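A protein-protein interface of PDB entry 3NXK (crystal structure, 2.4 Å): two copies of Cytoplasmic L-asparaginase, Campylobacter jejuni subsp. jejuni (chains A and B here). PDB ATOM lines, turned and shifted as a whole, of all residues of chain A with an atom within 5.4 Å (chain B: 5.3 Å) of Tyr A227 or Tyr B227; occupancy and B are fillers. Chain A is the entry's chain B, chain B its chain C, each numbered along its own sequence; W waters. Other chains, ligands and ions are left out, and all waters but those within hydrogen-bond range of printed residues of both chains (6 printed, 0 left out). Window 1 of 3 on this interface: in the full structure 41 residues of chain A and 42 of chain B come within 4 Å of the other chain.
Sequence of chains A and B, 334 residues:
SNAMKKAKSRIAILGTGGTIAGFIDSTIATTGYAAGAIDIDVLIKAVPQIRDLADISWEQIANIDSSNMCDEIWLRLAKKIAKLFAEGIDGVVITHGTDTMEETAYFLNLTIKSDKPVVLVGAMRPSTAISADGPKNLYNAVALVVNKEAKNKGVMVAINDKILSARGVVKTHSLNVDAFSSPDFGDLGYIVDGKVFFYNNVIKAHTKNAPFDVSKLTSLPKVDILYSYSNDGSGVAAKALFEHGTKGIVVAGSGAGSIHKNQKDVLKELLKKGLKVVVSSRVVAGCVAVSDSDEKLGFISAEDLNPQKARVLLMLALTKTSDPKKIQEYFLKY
NE2 of Gln B308 lies close to NE of Arg A282.
The side-chain hydroxyl of Tyr A229 sits at hydrogen-bond distance from the backbone NH of Ile B225 (3.2 Å).
The side-chain amide nitrogen (NE2) of Gln A308 sits close to the guanidinium group (NE) of Arg B282, 3.3 Å away.
The side-chain hydroxyl of Tyr B227 is in hydrogen-bond range of the side-chain amide oxygen of Gln A308.
The side-chain amide oxygen of Gln B308 is in hydrogen-bond range of the side-chain hydroxyl of Tyr A227, at 2.9 Å.
The backbone NH of Ile A225 is in hydrogen-bond range of the side-chain hydroxyl of Tyr B229 (3.3 Å).
OE1 of Gln A263 lies close to O of Tyr A227 (3.4 Å).
The guanidinium group of Arg B282 is in hydrogen-bond range of the backbone carbonyl oxygen of Ser B228, 2.9 Å away.
O of Ser A228 sits at hydrogen-bond distance from NH1 of Arg A282 (2.9 Å).
O of Tyr B227 lies within hydrogen-bond range of OG of Ser B234 (3.1 Å).
The side-chain amide oxygen (OE1) of Gln B263 lies close to the backbone carbonyl oxygen (O) of Tyr B227, 3.2 Å away.
O of Tyr A227 lies within hydrogen-bond range of OG of Ser A234 (3.1 Å).
Among the printed residues, pairs that only touch across the chains: Tyr A227 with Tyr B227, Tyr A227 with Pro B307, Tyr A227 with Ile B225, Pro A307 with Tyr B227 and Ile A225 with Tyr B227.
Tyr A227 touches four residues of chain B.
Of the printed residues of chain B, Arg A282 touches Gln B308 (3.4 Å).
Of the printed residues of chain A, Arg B282 touches Gln A308 (3.3 Å).
Of the printed residues of chain A, Pro B307 touches Tyr A227.
The nearest residue of chain B that does not touch Tyr A227 is Ala B252 (4.7 Å).
The nearest printed residue of chain A that does not touch Gln B308 is Tyr A229 (4.5 Å).
Of the 13 printed residues of chain A, 6 touch a printed residue of chain B.
Hydrophobic or aromatic side chains of chain A that line the printed part of chain B: Ile A225, Tyr A227, Tyr A229 and Pro A307.
Hydrophobic or aromatic side chains of chain B that line the printed part of chain A: Ile B225, Tyr B227, Tyr B229 and Pro B307.
Among the printed residues, 11 pairs touch across the chains.
Ile A225 touches Tyr B227, and with the chains exchanged Tyr A227 touches Ile B225.
Tyr A227 touches its own counterpart, Tyr B227.
Tyr A227 touches Pro B307, and with the chains exchanged Pro A307 touches Tyr B227.
Arg A282 touches Gln B308, and with the chains exchanged Gln A308 touches Arg B282.
Positions printed for both chains: 225, 226, 227, 228, 229, 232, 234, 251, 252, 263, 282, 307 and 308.
Water W3 lies within hydrogen-bond range of the side-chain hydroxyl (OG) of Ser A234 (2.5 Å), the backbone carbonyl oxygen (O) of Ile B225 (2.7 Å) and the backbone NH (N) of Tyr A227 (2.9 Å).
Water W2 lies within hydrogen-bond range of OH of Tyr B229, O of Ile A225 and OG of Ser B234.
Water W1 lies within hydrogen-bond range of the backbone carbonyl oxygen (O) of Arg B282 (2.8 Å) and the side-chain amide nitrogen (NE2) of Gln A308 (2.9 Å).
Water W6 lies within hydrogen-bond range of the side-chain hydroxyl (OG) of Ser A234 (2.8 Å), the side-chain hydroxyl (OH) of Tyr A229 (3.0 Å) and the backbone carbonyl oxygen (O) of Ile B225 (3.0 Å).
Water W5 bridges the backbone carbonyl oxygen (O) of Arg A282 and the side-chain amide nitrogen (NE2) of Gln B308.
Water W4 lies within hydrogen-bond range of the guanidinium group of Arg B282 (3.4 Å) and the side-chain amide nitrogen of Gln A308 (3.5 Å).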
ATOM      1  N   ILE A 225       7.966 -29.683  -8.139  1.00  0.00           N
ATOM      2  CA  ILE A 225       8.843 -28.530  -7.952  1.00  0.00           C
ATOM      3  C   ILE A 225       9.168 -28.283  -6.479  1.00  0.00           C
ATOM      4  O   ILE A 225       8.291 -28.335  -5.627  1.00  0.00           O
ATOM      5  CB  ILE A 225       8.235 -27.250  -8.557  1.00  0.00           C
ATOM      6  CG1 ILE A 225       7.743 -27.494  -9.989  1.00  0.00           C
ATOM      7  CG2 ILE A 225       9.228 -26.068  -8.478  1.00  0.00           C
ATOM      8  CD1 ILE A 225       7.046 -26.274 -10.599  1.00  0.00           C
ATOM      9  N   LEU A 226      10.438 -28.027  -6.195  1.00  0.00           N
ATOM     10  CA  LEU A 226      10.863 -27.625  -4.858  1.00  0.00           C
ATOM     11  C   LEU A 226      11.629 -26.302  -4.913  1.00  0.00           C
ATOM     12  O   LEU A 226      11.947 -25.787  -5.997  1.00  0.00           O
ATOM     13  CB  LEU A 226      11.722 -28.700  -4.193  1.00  0.00           C
ATOM     14  CG  LEU A 226      11.030 -30.033  -3.907  1.00  0.00           C
ATOM     15  CD1 LEU A 226      12.041 -31.161  -3.823  1.00  0.00           C
ATOM     16  CD2 LEU A 226      10.200 -29.967  -2.650  1.00  0.00           C
ATOM     17  N   TYR A 227      11.937 -25.789  -3.726  1.00  0.00           N
ATOM     18  CA  TYR A 227      12.457 -24.448  -3.531  1.00  0.00           C
ATOM     19  C   TYR A 227      13.702 -24.550  -2.677  1.00  0.00           C
ATOM     20  O   TYR A 227      13.793 -25.410  -1.808  1.00  0.00           O
ATOM     21  CB  TYR A 227      11.415 -23.642  -2.765  1.00  0.00           C
ATOM     22  CG  TYR A 227      11.395 -22.170  -3.072  1.00  0.00           C
ATOM     23  CD1 TYR A 227      10.692 -21.682  -4.166  1.00  0.00           C
ATOM     24  CD2 TYR A 227      12.045 -21.258  -2.255  1.00  0.00           C
ATOM     25  CE1 TYR A 227      10.658 -20.328  -4.450  1.00  0.00           C
ATOM     26  CE2 TYR A 227      12.008 -19.902  -2.536  1.00  0.00           C
ATOM     27  CZ  TYR A 227      11.315 -19.448  -3.634  1.00  0.00           C
ATOM     28  OH  TYR A 227      11.283 -18.108  -3.921  1.00  0.00           O
ATOM     29  N   SER A 228      14.670 -23.683  -2.915  1.00  0.00           N
ATOM     30  CA  SER A 228      15.867 -23.676  -2.080  1.00  0.00           C
ATOM     31  C   SER A 228      15.967 -22.354  -1.338  1.00  0.00           C
ATOM     32  O   SER A 228      15.572 -21.307  -1.855  1.00  0.00           O
ATOM     33  CB  SER A 228      17.150 -23.959  -2.878  1.00  0.00           C
ATOM     34  OG  SER A 228      18.277 -24.043  -2.006  1.00  0.00           O
ATOM     35  N   TYR A 229      16.481 -22.420  -0.114  1.00  0.00           N
ATOM     36  CA  TYR A 229      16.462 -21.293   0.795  1.00  0.00           C
ATOM     37  C   TYR A 229      17.387 -21.621   1.935  1.00  0.00           C
ATOM     38  O   TYR A 229      17.789 -22.780   2.093  1.00  0.00           O
ATOM     39  CB  TYR A 229      15.043 -21.035   1.331  1.00  0.00           C
ATOM     40  CG  TYR A 229      14.324 -22.273   1.845  1.00  0.00           C
ATOM     41  CD1 TYR A 229      14.365 -22.624   3.196  1.00  0.00           C
ATOM     42  CD2 TYR A 229      13.603 -23.092   0.979  1.00  0.00           C
ATOM     43  CE1 TYR A 229      13.706 -23.751   3.666  1.00  0.00           C
ATOM     44  CE2 TYR A 229      12.945 -24.227   1.437  1.00  0.00           C
ATOM     45  CZ  TYR A 229      12.999 -24.556   2.778  1.00  0.00           C
ATOM     46  OH  TYR A 229      12.342 -25.684   3.230  1.00  0.00           O
ATOM     47  N   ASP A 232      17.688 -24.838   4.138  1.00  0.00           N
ATOM     48  CA  ASP A 232      16.815 -25.681   3.323  1.00  0.00           C
ATOM     49  C   ASP A 232      16.467 -27.013   3.991  1.00  0.00           C
ATOM     50  O   ASP A 232      17.357 -27.760   4.382  1.00  0.00           O
ATOM     51  CB  ASP A 232      17.530 -25.949   2.004  1.00  0.00           C
ATOM     52  CG  ASP A 232      16.615 -26.443   0.921  1.00  0.00           C
ATOM     53  OD1 ASP A 232      15.569 -27.053   1.228  1.00  0.00           O
ATOM     54  OD2 ASP A 232      16.974 -26.224  -0.253  1.00  0.00           O
ATOM     55  N   SER A 234      14.240 -29.166   2.284  1.00  0.00           N
ATOM     56  CA  SER A 234      13.499 -29.798   1.189  1.00  0.00           C
ATOM     57  C   SER A 234      13.863 -31.261   0.904  1.00  0.00           C
ATOM     58  O   SER A 234      13.145 -31.949   0.169  1.00  0.00           O
ATOM     59  CB  SER A 234      13.651 -28.986  -0.095  1.00  0.00           C
ATOM     60  OG  SER A 234      12.924 -27.776   0.000  1.00  0.00           O
ATOM     61  N   VAL A 251      14.038 -27.734  -9.354  1.00  0.00           N
ATOM     62  CA  VAL A 251      14.367 -26.987  -8.147  1.00  0.00           C
ATOM     63  C   VAL A 251      14.494 -25.484  -8.387  1.00  0.00           C
ATOM     64  O   VAL A 251      15.273 -25.045  -9.237  1.00  0.00           O
ATOM     65  CB  VAL A 251      15.646 -27.532  -7.493  1.00  0.00           C
ATOM     66  CG1 VAL A 251      15.971 -26.747  -6.213  1.00  0.00           C
ATOM     67  CG2 VAL A 251      15.449 -29.005  -7.179  1.00  0.00           C
ATOM     68  N   ALA A 252      13.726 -24.693  -7.637  1.00  0.00           N
ATOM     69  CA  ALA A 252      13.868 -23.232  -7.696  1.00  0.00           C
ATOM     70  C   ALA A 252      15.067 -22.799  -6.854  1.00  0.00           C
ATOM     71  O   ALA A 252      14.932 -22.403  -5.686  1.00  0.00           O
ATOM     72  CB  ALA A 252      12.585 -22.536  -7.231  1.00  0.00           C
ATOM     73  N   GLN A 263      19.370 -30.001   0.811  1.00  0.00           N
ATOM     74  CA  GLN A 263      18.521 -30.599  -0.194  1.00  0.00           C
ATOM     75  C   GLN A 263      19.399 -31.262  -1.255  1.00  0.00           C
ATOM     76  O   GLN A 263      19.145 -32.391  -1.661  1.00  0.00           O
ATOM     77  CB  GLN A 263      17.602 -29.564  -0.799  1.00  0.00           C
ATOM     78  CG  GLN A 263      16.830 -30.063  -1.985  1.00  0.00           C
ATOM     79  CD  GLN A 263      15.970 -28.978  -2.605  1.00  0.00           C
ATOM     80  OE1 GLN A 263      16.114 -27.787  -2.291  1.00  0.00           O
ATOM     81  NE2 GLN A 263      15.065 -29.384  -3.486  1.00  0.00           N
ATOM     82  N   ARG A 282      14.709 -19.284  -8.253  1.00  0.00           N
ATOM     83  CA  ARG A 282      13.659 -18.443  -7.667  1.00  0.00           C
ATOM     84  C   ARG A 282      13.769 -16.990  -8.154  1.00  0.00           C
ATOM     85  O   ARG A 282      12.890 -16.151  -7.905  1.00  0.00           O
ATOM     86  CB  ARG A 282      13.738 -18.484  -6.145  1.00  0.00           C
ATOM     87  CG  ARG A 282      15.084 -18.031  -5.587  1.00  0.00           C
ATOM     88  CD  ARG A 282      15.156 -18.325  -4.107  1.00  0.00           C
ATOM     89  NE  ARG A 282      16.076 -17.427  -3.426  1.00  0.00           N
ATOM     90  CZ  ARG A 282      16.389 -17.511  -2.135  1.00  0.00           C
ATOM     91  NH1 ARG A 282      15.865 -18.456  -1.370  1.00  0.00           N
ATOM     92  NH2 ARG A 282      17.221 -16.629  -1.610  1.00  0.00           N
ATOM     93  N   PRO A 307      10.934 -22.128 -12.700  1.00  0.00           N
ATOM     94  CA  PRO A 307      10.562 -23.483 -12.246  1.00  0.00           C
ATOM     95  C   PRO A 307       9.366 -24.104 -12.969  1.00  0.00           C
ATOM     96  O   PRO A 307       9.459 -25.254 -13.434  1.00  0.00           O
ATOM     97  CB  PRO A 307      10.223 -23.275 -10.764  1.00  0.00           C
ATOM     98  CG  PRO A 307      11.151 -22.125 -10.351  1.00  0.00           C
ATOM     99  CD  PRO A 307      11.301 -21.238 -11.577  1.00  0.00           C
ATOM    100  N   GLN A 308       8.265 -23.358 -13.062  1.00  0.00           N
ATOM    101  CA  GLN A 308       7.009 -23.909 -13.554  1.00  0.00           C
ATOM    102  C   GLN A 308       7.016 -24.146 -15.064  1.00  0.00           C
ATOM    103  O   GLN A 308       6.401 -25.096 -15.553  1.00  0.00           O
ATOM    104  CB  GLN A 308       5.793 -23.068 -13.101  1.00  0.00           C
ATOM    105  CG  GLN A 308       5.807 -21.577 -13.481  1.00  0.00           C
ATOM    106  CD  GLN A 308       6.452 -20.679 -12.427  1.00  0.00           C
ATOM    107  OE1 GLN A 308       7.258 -21.126 -11.612  1.00  0.00           O
ATOM    108  NE2 GLN A 308       6.092 -19.413 -12.442  1.00  0.00           N
ATOM    109  N   ILE B 225       9.431 -24.333   2.882  1.00  0.00           N
ATOM    110  CA  ILE B 225       8.823 -23.620   1.769  1.00  0.00           C
ATOM    111  C   ILE B 225       8.373 -24.589   0.681  1.00  0.00           C
ATOM    112  O   ILE B 225       9.128 -25.487   0.306  1.00  0.00           O
ATOM    113  CB  ILE B 225       9.829 -22.630   1.163  1.00  0.00           C
ATOM    114  CG1 ILE B 225      10.412 -21.749   2.265  1.00  0.00           C
ATOM    115  CG2 ILE B 225       9.170 -21.800   0.072  1.00  0.00           C
ATOM    116  CD1 ILE B 225      11.364 -20.680   1.778  1.00  0.00           C
ATOM    117  N   LEU B 226       7.145 -24.414   0.195  1.00  0.00           N
ATOM    118  CA  LEU B 226       6.636 -25.185  -0.947  1.00  0.00           C
ATOM    119  C   LEU B 226       6.119 -24.256  -2.033  1.00  0.00           C
ATOM    120  O   LEU B 226       5.862 -23.077  -1.789  1.00  0.00           O
ATOM    121  CB  LEU B 226       5.501 -26.117  -0.540  1.00  0.00           C
ATOM    122  CG  LEU B 226       5.848 -27.233   0.438  1.00  0.00           C
ATOM    123  CD1 LEU B 226       4.547 -27.876   0.942  1.00  0.00           C
ATOM    124  CD2 LEU B 226       6.752 -28.261  -0.236  1.00  0.00           C
ATOM    125  N   TYR B 227       5.953 -24.811  -3.222  1.00  0.00           N
ATOM    126  CA  TYR B 227       5.698 -24.040  -4.424  1.00  0.00           C
ATOM    127  C   TYR B 227       4.344 -24.503  -4.958  1.00  0.00           C
ATOM    128  O   TYR B 227       3.943 -25.638  -4.716  1.00  0.00           O
ATOM    129  CB  TYR B 227       6.808 -24.365  -5.429  1.00  0.00           C
ATOM    130  CG  TYR B 227       7.110 -23.294  -6.459  1.00  0.00           C
ATOM    131  CD1 TYR B 227       7.937 -22.221  -6.159  1.00  0.00           C
ATOM    132  CD2 TYR B 227       6.598 -23.381  -7.746  1.00  0.00           C
ATOM    133  CE1 TYR B 227       8.222 -21.256  -7.104  1.00  0.00           C
ATOM    134  CE2 TYR B 227       6.883 -22.411  -8.699  1.00  0.00           C
ATOM    135  CZ  TYR B 227       7.689 -21.354  -8.376  1.00  0.00           C
ATOM    136  OH  TYR B 227       7.957 -20.396  -9.337  1.00  0.00           O
ATOM    137  N   SER B 228       3.623 -23.646  -5.671  1.00  0.00           N
ATOM    138  CA  SER B 228       2.375 -24.098  -6.297  1.00  0.00           C
ATOM    139  C   SER B 228       2.409 -23.937  -7.807  1.00  0.00           C
ATOM    140  O   SER B 228       2.953 -22.973  -8.320  1.00  0.00           O
ATOM    141  CB  SER B 228       1.154 -23.388  -5.722  1.00  0.00           C
ATOM    142  OG  SER B 228      -0.033 -23.863  -6.354  1.00  0.00           O
ATOM    143  N   TYR B 229       1.818 -24.894  -8.513  1.00  0.00           N
ATOM    144  CA  TYR B 229       1.884 -24.939  -9.968  1.00  0.00           C
ATOM    145  C   TYR B 229       0.781 -25.865 -10.513  1.00  0.00           C
ATOM    146  O   TYR B 229       0.069 -26.519  -9.751  1.00  0.00           O
ATOM    147  CB  TYR B 229       3.273 -25.426 -10.399  1.00  0.00           C
ATOM    148  CG  TYR B 229       3.698 -26.650  -9.626  1.00  0.00           C
ATOM    149  CD1 TYR B 229       3.456 -27.926 -10.129  1.00  0.00           C
ATOM    150  CD2 TYR B 229       4.298 -26.537  -8.369  1.00  0.00           C
ATOM    151  CE1 TYR B 229       3.806 -29.056  -9.411  1.00  0.00           C
ATOM    152  CE2 TYR B 229       4.644 -27.665  -7.637  1.00  0.00           C
ATOM    153  CZ  TYR B 229       4.392 -28.920  -8.167  1.00  0.00           C
ATOM    154  OH  TYR B 229       4.745 -30.046  -7.468  1.00  0.00           O
ATOM    155  N   ASP B 232      -0.419 -29.591  -9.400  1.00  0.00           N
ATOM    156  CA  ASP B 232       0.487 -29.523  -8.257  1.00  0.00           C
ATOM    157  C   ASP B 232       0.505 -30.852  -7.482  1.00  0.00           C
ATOM    158  O   ASP B 232      -0.541 -31.406  -7.157  1.00  0.00           O
ATOM    159  CB  ASP B 232       0.046 -28.329  -7.389  1.00  0.00           C
ATOM    160  CG  ASP B 232       0.861 -28.155  -6.115  1.00  0.00           C
ATOM    161  OD1 ASP B 232       1.648 -29.055  -5.749  1.00  0.00           O
ATOM    162  OD2 ASP B 232       0.673 -27.103  -5.456  1.00  0.00           O
ATOM    163  N   SER B 234       2.411 -31.140  -4.567  1.00  0.00           N
ATOM    164  CA  SER B 234       3.051 -30.787  -3.291  1.00  0.00           C
ATOM    165  C   SER B 234       2.370 -31.302  -2.029  1.00  0.00           C
ATOM    166  O   SER B 234       2.990 -31.330  -0.963  1.00  0.00           O
ATOM    167  CB  SER B 234       3.200 -29.271  -3.174  1.00  0.00           C
ATOM    168  OG  SER B 234       3.928 -28.753  -4.270  1.00  0.00           O
ATOM    169  N   VAL B 251       4.038 -21.202   1.531  1.00  0.00           N
ATOM    170  CA  VAL B 251       3.698 -21.603   0.172  1.00  0.00           C
ATOM    171  C   VAL B 251       3.885 -20.454  -0.826  1.00  0.00           C
ATOM    172  O   VAL B 251       3.387 -19.353  -0.614  1.00  0.00           O
ATOM    173  CB  VAL B 251       2.239 -22.126   0.059  1.00  0.00           C
ATOM    174  CG1 VAL B 251       1.991 -22.694  -1.343  1.00  0.00           C
ATOM    175  CG2 VAL B 251       1.962 -23.182   1.114  1.00  0.00           C
ATOM    176  N   ALA B 252       4.609 -20.719  -1.907  1.00  0.00           N
ATOM    177  CA  ALA B 252       4.722 -19.762  -3.003  1.00  0.00           C
ATOM    178  C   ALA B 252       3.574 -19.986  -3.969  1.00  0.00           C
ATOM    179  O   ALA B 252       3.679 -20.780  -4.895  1.00  0.00           O
ATOM    180  CB  ALA B 252       6.058 -19.929  -3.725  1.00  0.00           C
ATOM    181  N   GLN B 263      -2.767 -29.333  -3.233  1.00  0.00           N
ATOM    182  CA  GLN B 263      -1.949 -28.993  -2.074  1.00  0.00           C
ATOM    183  C   GLN B 263      -2.792 -28.400  -0.942  1.00  0.00           C
ATOM    184  O   GLN B 263      -2.644 -28.779   0.221  1.00  0.00           O
ATOM    185  CB  GLN B 263      -0.817 -28.020  -2.458  1.00  0.00           C
ATOM    186  CG  GLN B 263      -0.126 -27.407  -1.239  1.00  0.00           C
ATOM    187  CD  GLN B 263       1.198 -26.739  -1.549  1.00  0.00           C
ATOM    188  OE1 GLN B 263       1.598 -26.598  -2.709  1.00  0.00           O
ATOM    189  NE2 GLN B 263       1.890 -26.326  -0.501  1.00  0.00           N
ATOM    190  N   ARG B 282       4.914 -16.631  -5.915  1.00  0.00           N
ATOM    191  CA  ARG B 282       6.030 -16.987  -6.780  1.00  0.00           C
ATOM    192  C   ARG B 282       6.226 -15.865  -7.784  1.00  0.00           C
ATOM    193  O   ARG B 282       7.203 -15.853  -8.528  1.00  0.00           O
ATOM    194  CB  ARG B 282       5.699 -18.273  -7.530  1.00  0.00           C
ATOM    195  CG  ARG B 282       4.546 -18.107  -8.517  1.00  0.00           C
ATOM    196  CD  ARG B 282       4.167 -19.422  -9.126  1.00  0.00           C
ATOM    197  NE  ARG B 282       3.473 -19.260 -10.394  1.00  0.00           N
ATOM    198  CZ  ARG B 282       3.110 -20.273 -11.173  1.00  0.00           C
ATOM    199  NH1 ARG B 282       3.385 -21.529 -10.816  1.00  0.00           N
ATOM    200  NH2 ARG B 282       2.494 -20.034 -12.318  1.00  0.00           N
ATOM    201  N   PRO B 307       8.702 -15.662  -0.714  1.00  0.00           N
ATOM    202  CA  PRO B 307       8.620 -16.835   0.158  1.00  0.00           C
ATOM    203  C   PRO B 307       9.750 -16.908   1.191  1.00  0.00           C
ATOM    204  O   PRO B 307       9.489 -17.098   2.379  1.00  0.00           O
ATOM    205  CB  PRO B 307       8.667 -18.011  -0.833  1.00  0.00           C
ATOM    206  CG  PRO B 307       8.114 -17.432  -2.104  1.00  0.00           C
ATOM    207  CD  PRO B 307       8.624 -16.009  -2.141  1.00  0.00           C
ATOM    208  N   GLN B 308      10.987 -16.755   0.739  1.00  0.00           N
ATOM    209  CA  GLN B 308      12.141 -16.908   1.618  1.00  0.00           C
ATOM    210  C   GLN B 308      12.200 -15.830   2.703  1.00  0.00           C
ATOM    211  O   GLN B 308      12.647 -16.085   3.822  1.00  0.00           O
ATOM    212  CB  GLN B 308      13.438 -16.914   0.802  1.00  0.00           C
ATOM    213  CG  GLN B 308      13.614 -15.719  -0.101  1.00  0.00           C
ATOM    214  CD  GLN B 308      12.978 -15.919  -1.456  1.00  0.00           C
ATOM    215  OE1 GLN B 308      11.940 -16.566  -1.583  1.00  0.00           O
ATOM    216  NE2 GLN B 308      13.606 -15.362  -2.486  1.00  0.00           N
HETATM  217  O   HOH W   1       7.220 -17.125 -11.006  1.00  0.00           O
HETATM  218  O   HOH W   2       6.278 -30.466  -5.218  1.00  0.00           O
HETATM  219  O   HOH W   3      10.919 -26.844  -1.256  1.00  0.00           O
HETATM  220  O   HOH W   4       4.360 -16.409 -12.092  1.00  0.00           O
HETATM  221  O   HOH W   5      12.448 -14.834  -5.308  1.00  0.00           O
HETATM  222  O   HOH W   6      10.684 -27.641   1.694  1.00  0.00           O
